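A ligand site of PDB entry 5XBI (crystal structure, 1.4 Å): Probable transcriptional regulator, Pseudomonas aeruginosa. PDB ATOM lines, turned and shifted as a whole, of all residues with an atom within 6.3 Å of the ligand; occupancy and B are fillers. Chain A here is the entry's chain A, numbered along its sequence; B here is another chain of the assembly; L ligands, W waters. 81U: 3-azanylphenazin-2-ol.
A nitrogen (NAI) of the ligand is in hydrogen-bond range of the side-chain carboxylate (OE1) of Glu 130 (2.7 Å).
The side-chain hydroxyl (OH) of Tyr 132 sits at hydrogen-bond distance from a nitrogen (NAA) of the ligand (3.1 Å).
The side-chain hydroxyl (OH) of Tyr 66 is in hydrogen-bond range of the indole nitrogen (NE1) of Trp 33.
The backbone NH (N) of Ala 101 lies within hydrogen-bond range of the backbone carbonyl oxygen (O) of Pro 139 (2.7 Å).
The side-chain hydroxyl (OH) of Tyr 132 is in hydrogen-bond range of the side-chain carboxylate (OE2) of Glu 130 (2.6 Å).
The side-chain hydroxyl (OH) of Tyr 66 sits at hydrogen-bond distance from the side-chain carboxylate (OE2) of Glu 130 (2.6 Å).
The side-chain sulfur (SG) of Cys 56 sits at hydrogen-bond distance from the side-chain carboxylate (OE1) of Glu 130 (3.7 Å).
Ile 29 touches the ligand (CG2 to CAL, 3.5 Å).
Gly 30 touches the ligand.
Trp 33 touches the ligand.
SG of Cys 56 touches CAE of the ligand, at 3.8 Å.
Tyr 66 touches the ligand (OH to CAG, 3.7 Å).
CB of Ala 101 touches NAA of the ligand, 3.3 Å away.
Ile 104 touches the ligand (CG2 to NAI, 3.9 Å).
CB of Ala 105 of chain A touches CAF of the ligand, 3.5 Å away.
Phe 108 touches the ligand.
O of Ala 105 of chain B touches CAD of the ligand, 3.5 Å away.
Glu 106 of chain B touches the ligand.
Hydrophobic or aromatic side chains that line the ligand: Ile 29, Trp 33, Ala 101, Ile 104, Ala 105 of chain A, Phe 108 and Ala 105 of chain B.
Of the 21 residues printed, 13 come within 4 Å of the ligand.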
ATOM      1  N   ILE A  29     -18.088 -14.661  24.091  1.00  0.00           N
ATOM      2  CA  ILE A  29     -17.706 -15.366  22.875  1.00  0.00           C
ATOM      3  C   ILE A  29     -16.367 -16.080  23.070  1.00  0.00           C
ATOM      4  O   ILE A  29     -16.164 -17.195  22.582  1.00  0.00           O
ATOM      5  CB  ILE A  29     -17.715 -14.413  21.663  1.00  0.00           C
ATOM      6  CG1 ILE A  29     -19.149 -13.947  21.377  1.00  0.00           C
ATOM      7  CG2 ILE A  29     -17.095 -15.077  20.441  1.00  0.00           C
ATOM      8  CD1 ILE A  29     -19.242 -12.844  20.325  1.00  0.00           C
ATOM      9  N   GLY A  30     -15.441 -15.427  23.767  1.00  0.00           N
ATOM     10  CA  GLY A  30     -14.157 -16.069  24.031  1.00  0.00           C
ATOM     11  C   GLY A  30     -14.292 -17.324  24.865  1.00  0.00           C
ATOM     12  O   GLY A  30     -13.615 -18.322  24.616  1.00  0.00           O
ATOM     13  N   TRP A  33     -15.655 -20.212  22.558  1.00  0.00           N
ATOM     14  CA  TRP A  33     -14.610 -20.896  21.797  1.00  0.00           C
ATOM     15  C   TRP A  33     -13.764 -21.792  22.693  1.00  0.00           C
ATOM     16  O   TRP A  33     -13.417 -22.904  22.309  1.00  0.00           O
ATOM     17  CB  TRP A  33     -13.739 -19.890  21.053  1.00  0.00           C
ATOM     18  CG  TRP A  33     -14.364 -19.381  19.784  1.00  0.00           C
ATOM     19  CD1 TRP A  33     -14.894 -18.148  19.569  1.00  0.00           C
ATOM     20  CD2 TRP A  33     -14.512 -20.113  18.553  1.00  0.00           C
ATOM     21  NE1 TRP A  33     -15.384 -18.064  18.290  1.00  0.00           N
ATOM     22  CE2 TRP A  33     -15.140 -19.252  17.638  1.00  0.00           C
ATOM     23  CE3 TRP A  33     -14.160 -21.403  18.144  1.00  0.00           C
ATOM     24  CZ2 TRP A  33     -15.442 -19.626  16.335  1.00  0.00           C
ATOM     25  CZ3 TRP A  33     -14.462 -21.776  16.840  1.00  0.00           C
ATOM     26  CH2 TRP A  33     -15.093 -20.901  15.951  1.00  0.00           C
ATOM     27  N   CYS A  56     -22.493 -14.672  13.094  1.00  0.00           N
ATOM     28  CA  CYS A  56     -23.095 -13.532  13.782  1.00  0.00           C
ATOM     29  C   CYS A  56     -24.493 -13.374  13.216  1.00  0.00           C
ATOM     30  O   CYS A  56     -24.675 -12.893  12.089  1.00  0.00           O
ATOM     31  CB  CYS A  56     -22.265 -12.267  13.556  1.00  0.00           C
ATOM     32  SG  CYS A  56     -20.634 -12.349  14.295  1.00  0.00           S
ATOM     33  N   PHE A  64     -28.461 -10.412  19.775  1.00  0.00           N
ATOM     34  CA  PHE A  64     -27.282 -10.944  19.104  1.00  0.00           C
ATOM     35  C   PHE A  64     -27.144 -12.436  19.407  1.00  0.00           C
ATOM     36  O   PHE A  64     -27.314 -12.872  20.546  1.00  0.00           O
ATOM     37  CB  PHE A  64     -26.072 -10.158  19.619  1.00  0.00           C
ATOM     38  CG  PHE A  64     -24.760 -10.578  19.025  1.00  0.00           C
ATOM     39  CD1 PHE A  64     -24.300 -10.026  17.834  1.00  0.00           C
ATOM     40  CD2 PHE A  64     -23.958 -11.500  19.684  1.00  0.00           C
ATOM     41  CE1 PHE A  64     -23.082 -10.406  17.303  1.00  0.00           C
ATOM     42  CE2 PHE A  64     -22.753 -11.887  19.152  1.00  0.00           C
ATOM     43  CZ  PHE A  64     -22.302 -11.336  17.972  1.00  0.00           C
ATOM     44  N   TYR A  66     -24.676 -15.898  18.388  1.00  0.00           N
ATOM     45  CA  TYR A  66     -23.410 -16.298  17.804  1.00  0.00           C
ATOM     46  C   TYR A  66     -23.276 -17.812  17.859  1.00  0.00           C
ATOM     47  O   TYR A  66     -23.650 -18.441  18.859  1.00  0.00           O
ATOM     48  CB  TYR A  66     -22.258 -15.623  18.573  1.00  0.00           C
ATOM     49  CG  TYR A  66     -20.853 -15.810  18.014  1.00  0.00           C
ATOM     50  CD1 TYR A  66     -20.109 -16.946  18.315  1.00  0.00           C
ATOM     51  CD2 TYR A  66     -20.262 -14.822  17.235  1.00  0.00           C
ATOM     52  CE1 TYR A  66     -18.816 -17.094  17.841  1.00  0.00           C
ATOM     53  CE2 TYR A  66     -18.979 -14.968  16.762  1.00  0.00           C
ATOM     54  CZ  TYR A  66     -18.250 -16.092  17.079  1.00  0.00           C
ATOM     55  OH  TYR A  66     -16.966 -16.241  16.616  1.00  0.00           O
ATOM     56  N   ALA A 101      -8.545 -12.134  17.557  1.00  0.00           N
ATOM     57  CA  ALA A 101      -9.968 -12.453  17.536  1.00  0.00           C
ATOM     58  C   ALA A 101     -10.819 -11.413  18.256  1.00  0.00           C
ATOM     59  O   ALA A 101     -11.844 -11.003  17.685  1.00  0.00           O
ATOM     60  CB  ALA A 101     -10.219 -13.883  18.050  1.00  0.00           C
ATOM     61  N   PRO A 102     -10.466 -10.923  19.445  1.00  0.00           N
ATOM     62  CA  PRO A 102     -11.277  -9.846  20.036  1.00  0.00           C
ATOM     63  C   PRO A 102     -11.330  -8.587  19.189  1.00  0.00           C
ATOM     64  O   PRO A 102     -12.316  -7.852  19.276  1.00  0.00           O
ATOM     65  CB  PRO A 102     -10.600  -9.596  21.395  1.00  0.00           C
ATOM     66  CG  PRO A 102      -9.927 -10.870  21.721  1.00  0.00           C
ATOM     67  CD  PRO A 102      -9.449 -11.411  20.403  1.00  0.00           C
ATOM     68  N   GLN A 103     -10.320  -8.333  18.361  1.00  0.00           N
ATOM     69  CA  GLN A 103     -10.350  -7.165  17.472  1.00  0.00           C
ATOM     70  C   GLN A 103     -11.285  -7.347  16.284  1.00  0.00           C
ATOM     71  O   GLN A 103     -11.554  -6.377  15.563  1.00  0.00           O
ATOM     72  CB  GLN A 103      -8.946  -6.800  16.983  1.00  0.00           C
ATOM     73  CG  GLN A 103      -8.045  -6.209  18.063  1.00  0.00           C
ATOM     74  CD  GLN A 103      -6.629  -5.966  17.576  1.00  0.00           C
ATOM     75  OE1 GLN A 103      -6.119  -6.683  16.714  1.00  0.00           O
ATOM     76  NE2 GLN A 103      -5.991  -4.953  18.138  1.00  0.00           N
ATOM     77  N   ILE A 104     -11.830  -8.553  16.063  1.00  0.00           N
ATOM     78  CA  ILE A 104     -12.815  -8.724  14.998  1.00  0.00           C
ATOM     79  C   ILE A 104     -13.959  -7.753  15.173  1.00  0.00           C
ATOM     80  O   ILE A 104     -14.471  -7.189  14.197  1.00  0.00           O
ATOM     81  CB  ILE A 104     -13.316 -10.184  14.976  1.00  0.00           C
ATOM     82  CG1 ILE A 104     -12.205 -11.116  14.479  1.00  0.00           C
ATOM     83  CG2 ILE A 104     -14.579 -10.274  14.130  1.00  0.00           C
ATOM     84  CD1 ILE A 104     -12.505 -12.596  14.697  1.00  0.00           C
ATOM     85  N   ALA A 105     -14.380  -7.532  16.417  1.00  0.00           N
ATOM     86  CA  ALA A 105     -15.479  -6.631  16.714  1.00  0.00           C
ATOM     87  C   ALA A 105     -15.188  -5.216  16.213  1.00  0.00           C
ATOM     88  O   ALA A 105     -16.090  -4.520  15.722  1.00  0.00           O
ATOM     89  CB  ALA A 105     -15.661  -6.587  18.218  1.00  0.00           C
ATOM     90  N   PHE A 108     -15.665  -5.243  12.423  1.00  0.00           N
ATOM     91  CA  PHE A 108     -17.084  -5.157  12.088  1.00  0.00           C
ATOM     92  C   PHE A 108     -17.586  -3.722  12.188  1.00  0.00           C
ATOM     93  O   PHE A 108     -18.332  -3.254  11.327  1.00  0.00           O
ATOM     94  CB  PHE A 108     -17.927  -6.064  12.988  1.00  0.00           C
ATOM     95  CG  PHE A 108     -18.143  -7.449  12.429  1.00  0.00           C
ATOM     96  CD1 PHE A 108     -18.958  -7.671  11.333  1.00  0.00           C
ATOM     97  CD2 PHE A 108     -17.575  -8.545  13.063  1.00  0.00           C
ATOM     98  CE1 PHE A 108     -19.165  -8.941  10.852  1.00  0.00           C
ATOM     99  CE2 PHE A 108     -17.785  -9.821  12.570  1.00  0.00           C
ATOM    100  CZ  PHE A 108     -18.583 -10.015  11.471  1.00  0.00           C
ATOM    101  N   GLU A 130     -17.658 -14.911  10.518  1.00  0.00           N
ATOM    102  CA  GLU A 130     -16.210 -14.969  10.543  1.00  0.00           C
ATOM    103  C   GLU A 130     -15.771 -16.315   9.983  1.00  0.00           C
ATOM    104  O   GLU A 130     -16.351 -17.351  10.324  1.00  0.00           O
ATOM    105  CB  GLU A 130     -15.727 -14.852  11.992  1.00  0.00           C
ATOM    106  CG  GLU A 130     -16.138 -13.544  12.654  1.00  0.00           C
ATOM    107  CD  GLU A 130     -16.424 -13.701  14.135  1.00  0.00           C
ATOM    108  OE1 GLU A 130     -17.026 -12.772  14.693  1.00  0.00           O
ATOM    109  OE2 GLU A 130     -16.044 -14.732  14.732  1.00  0.00           O
ATOM    110  N   TYR A 132     -12.541 -18.741   9.618  1.00  0.00           N
ATOM    111  CA  TYR A 132     -11.232 -19.021  10.206  1.00  0.00           C
ATOM    112  C   TYR A 132     -10.607 -20.186   9.434  1.00  0.00           C
ATOM    113  O   TYR A 132     -11.105 -21.305   9.500  1.00  0.00           O
ATOM    114  CB  TYR A 132     -11.368 -19.415  11.682  1.00  0.00           C
ATOM    115  CG  TYR A 132     -11.992 -18.393  12.608  1.00  0.00           C
ATOM    116  CD1 TYR A 132     -13.369 -18.307  12.786  1.00  0.00           C
ATOM    117  CD2 TYR A 132     -11.195 -17.532  13.351  1.00  0.00           C
ATOM    118  CE1 TYR A 132     -13.932 -17.383  13.654  1.00  0.00           C
ATOM    119  CE2 TYR A 132     -11.748 -16.613  14.228  1.00  0.00           C
ATOM    120  CZ  TYR A 132     -13.111 -16.532  14.371  1.00  0.00           C
ATOM    121  OH  TYR A 132     -13.636 -15.590  15.252  1.00  0.00           O
ATOM    122  N   PHE A 136      -5.499 -18.305  10.457  1.00  0.00           N
ATOM    123  CA  PHE A 136      -5.767 -17.976  11.848  1.00  0.00           C
ATOM    124  C   PHE A 136      -4.806 -18.770  12.724  1.00  0.00           C
ATOM    125  O   PHE A 136      -4.823 -20.008  12.721  1.00  0.00           O
ATOM    126  CB  PHE A 136      -7.219 -18.320  12.200  1.00  0.00           C
ATOM    127  CG  PHE A 136      -7.581 -18.017  13.623  1.00  0.00           C
ATOM    128  CD1 PHE A 136      -7.736 -16.703  14.054  1.00  0.00           C
ATOM    129  CD2 PHE A 136      -7.770 -19.034  14.547  1.00  0.00           C
ATOM    130  CE1 PHE A 136      -8.071 -16.431  15.370  1.00  0.00           C
ATOM    131  CE2 PHE A 136      -8.108 -18.767  15.851  1.00  0.00           C
ATOM    132  CZ  PHE A 136      -8.257 -17.462  16.269  1.00  0.00           C
ATOM    133  N   PRO A 139      -6.150 -16.944  18.916  1.00  0.00           N
ATOM    134  CA  PRO A 139      -7.052 -15.808  19.176  1.00  0.00           C
ATOM    135  C   PRO A 139      -6.357 -14.502  19.532  1.00  0.00           C
ATOM    136  O   PRO A 139      -6.930 -13.433  19.290  1.00  0.00           O
ATOM    137  CB  PRO A 139      -7.944 -16.310  20.325  1.00  0.00           C
ATOM    138  CG  PRO A 139      -7.166 -17.430  20.944  1.00  0.00           C
ATOM    139  CD  PRO A 139      -6.397 -18.074  19.841  1.00  0.00           C
ATOM    140  N   PRO B 102     -17.304  -4.975  27.053  1.00  0.00           N
ATOM    141  CA  PRO B 102     -16.902  -5.748  25.867  1.00  0.00           C
ATOM    142  C   PRO B 102     -18.077  -6.149  24.998  1.00  0.00           C
ATOM    143  O   PRO B 102     -17.922  -6.236  23.778  1.00  0.00           O
ATOM    144  CB  PRO B 102     -16.203  -6.971  26.471  1.00  0.00           C
ATOM    145  CG  PRO B 102     -15.690  -6.494  27.768  1.00  0.00           C
ATOM    146  CD  PRO B 102     -16.719  -5.538  28.287  1.00  0.00           C
ATOM    147  N   ALA B 105     -19.503  -4.225  21.574  1.00  0.00           N
ATOM    148  CA  ALA B 105     -19.165  -4.627  20.216  1.00  0.00           C
ATOM    149  C   ALA B 105     -20.287  -5.433  19.572  1.00  0.00           C
ATOM    150  O   ALA B 105     -20.550  -5.288  18.377  1.00  0.00           O
ATOM    151  CB  ALA B 105     -17.916  -5.491  20.276  1.00  0.00           C
ATOM    152  N   GLU B 106     -20.910  -6.306  20.359  1.00  0.00           N
ATOM    153  CA  GLU B 106     -22.002  -7.114  19.837  1.00  0.00           C
ATOM    154  C   GLU B 106     -23.202  -6.247  19.500  1.00  0.00           C
ATOM    155  O   GLU B 106     -23.855  -6.449  18.471  1.00  0.00           O
ATOM    156  CB  GLU B 106     -22.369  -8.166  20.871  1.00  0.00           C
ATOM    157  CG  GLU B 106     -21.232  -9.134  21.097  1.00  0.00           C
ATOM    158  CD  GLU B 106     -21.333  -9.905  22.387  1.00  0.00           C
ATOM    159  OE1 GLU B 106     -20.278 -10.378  22.852  1.00  0.00           O
ATOM    160  OE2 GLU B 106     -22.451 -10.038  22.947  1.00  0.00           O
ATOM    161  N   SER B 107     -23.490  -5.242  20.340  1.00  0.00           N
ATOM    162  CA  SER B 107     -24.574  -4.313  20.044  1.00  0.00           C
ATOM    163  C   SER B 107     -24.293  -3.505  18.782  1.00  0.00           C
ATOM    164  O   SER B 107     -25.201  -3.306  17.965  1.00  0.00           O
ATOM    165  CB  SER B 107     -24.861  -3.413  21.240  1.00  0.00           C
ATOM    166  OG  SER B 107     -25.535  -4.134  22.258  1.00  0.00           O
ATOM    167  N   GLN B 109     -22.606  -4.472  16.181  1.00  0.00           N
ATOM    168  CA  GLN B 109     -22.814  -5.342  15.038  1.00  0.00           C
ATOM    169  C   GLN B 109     -24.295  -5.578  14.795  1.00  0.00           C
ATOM    170  O   GLN B 109     -24.756  -5.596  13.650  1.00  0.00           O
ATOM    171  CB  GLN B 109     -22.045  -6.647  15.230  1.00  0.00           C
ATOM    172  CG  GLN B 109     -21.964  -7.532  13.963  1.00  0.00           C
ATOM    173  CD  GLN B 109     -23.242  -8.324  13.683  1.00  0.00           C
ATOM    174  OE1 GLN B 109     -24.050  -8.573  14.590  1.00  0.00           O
ATOM    175  NE2 GLN B 109     -23.439  -8.718  12.417  1.00  0.00           N
HETATM  176  OAB 81U L   1     -13.238 -13.815  20.900  1.00  0.00           O
HETATM  177  CAL 81U L   1     -14.107 -13.271  19.937  1.00  0.00           C
HETATM  178  CAH 81U L   1     -14.901 -12.167  20.272  1.00  0.00           C
HETATM  179  CAP 81U L   1     -15.784 -11.624  19.289  1.00  0.00           C
HETATM  180  NAJ 81U L   1     -16.576 -10.532  19.589  1.00  0.00           N
HETATM  181  CAN 81U L   1     -17.422 -10.028  18.632  1.00  0.00           C
HETATM  182  CAF 81U L   1     -18.253  -8.909  18.912  1.00  0.00           C
HETATM  183  CAD 81U L   1     -19.095  -8.408  17.923  1.00  0.00           C
HETATM  184  CAC 81U L   1     -19.140  -8.999  16.665  1.00  0.00           C
HETATM  185  CAE 81U L   1     -18.336 -10.099  16.382  1.00  0.00           C
HETATM  186  CAM 81U L   1     -17.474 -10.611  17.388  1.00  0.00           C
HETATM  187  NAI 81U L   1     -16.673 -11.679  17.106  1.00  0.00           N
HETATM  188  CAO 81U L   1     -15.840 -12.183  18.042  1.00  0.00           C
HETATM  189  CAG 81U L   1     -15.031 -13.313  17.708  1.00  0.00           C
HETATM  190  CAK 81U L   1     -14.174 -13.849  18.654  1.00  0.00           C
HETATM  191  NAA 81U L   1     -13.361 -15.000  18.312  1.00  0.00           N
HETATM  192  O   HOH W   1     -14.133  -9.351  18.323  1.00  0.00           O
HETATM  193  O   HOH W   2     -17.499  -9.161  22.126  1.00  0.00           O
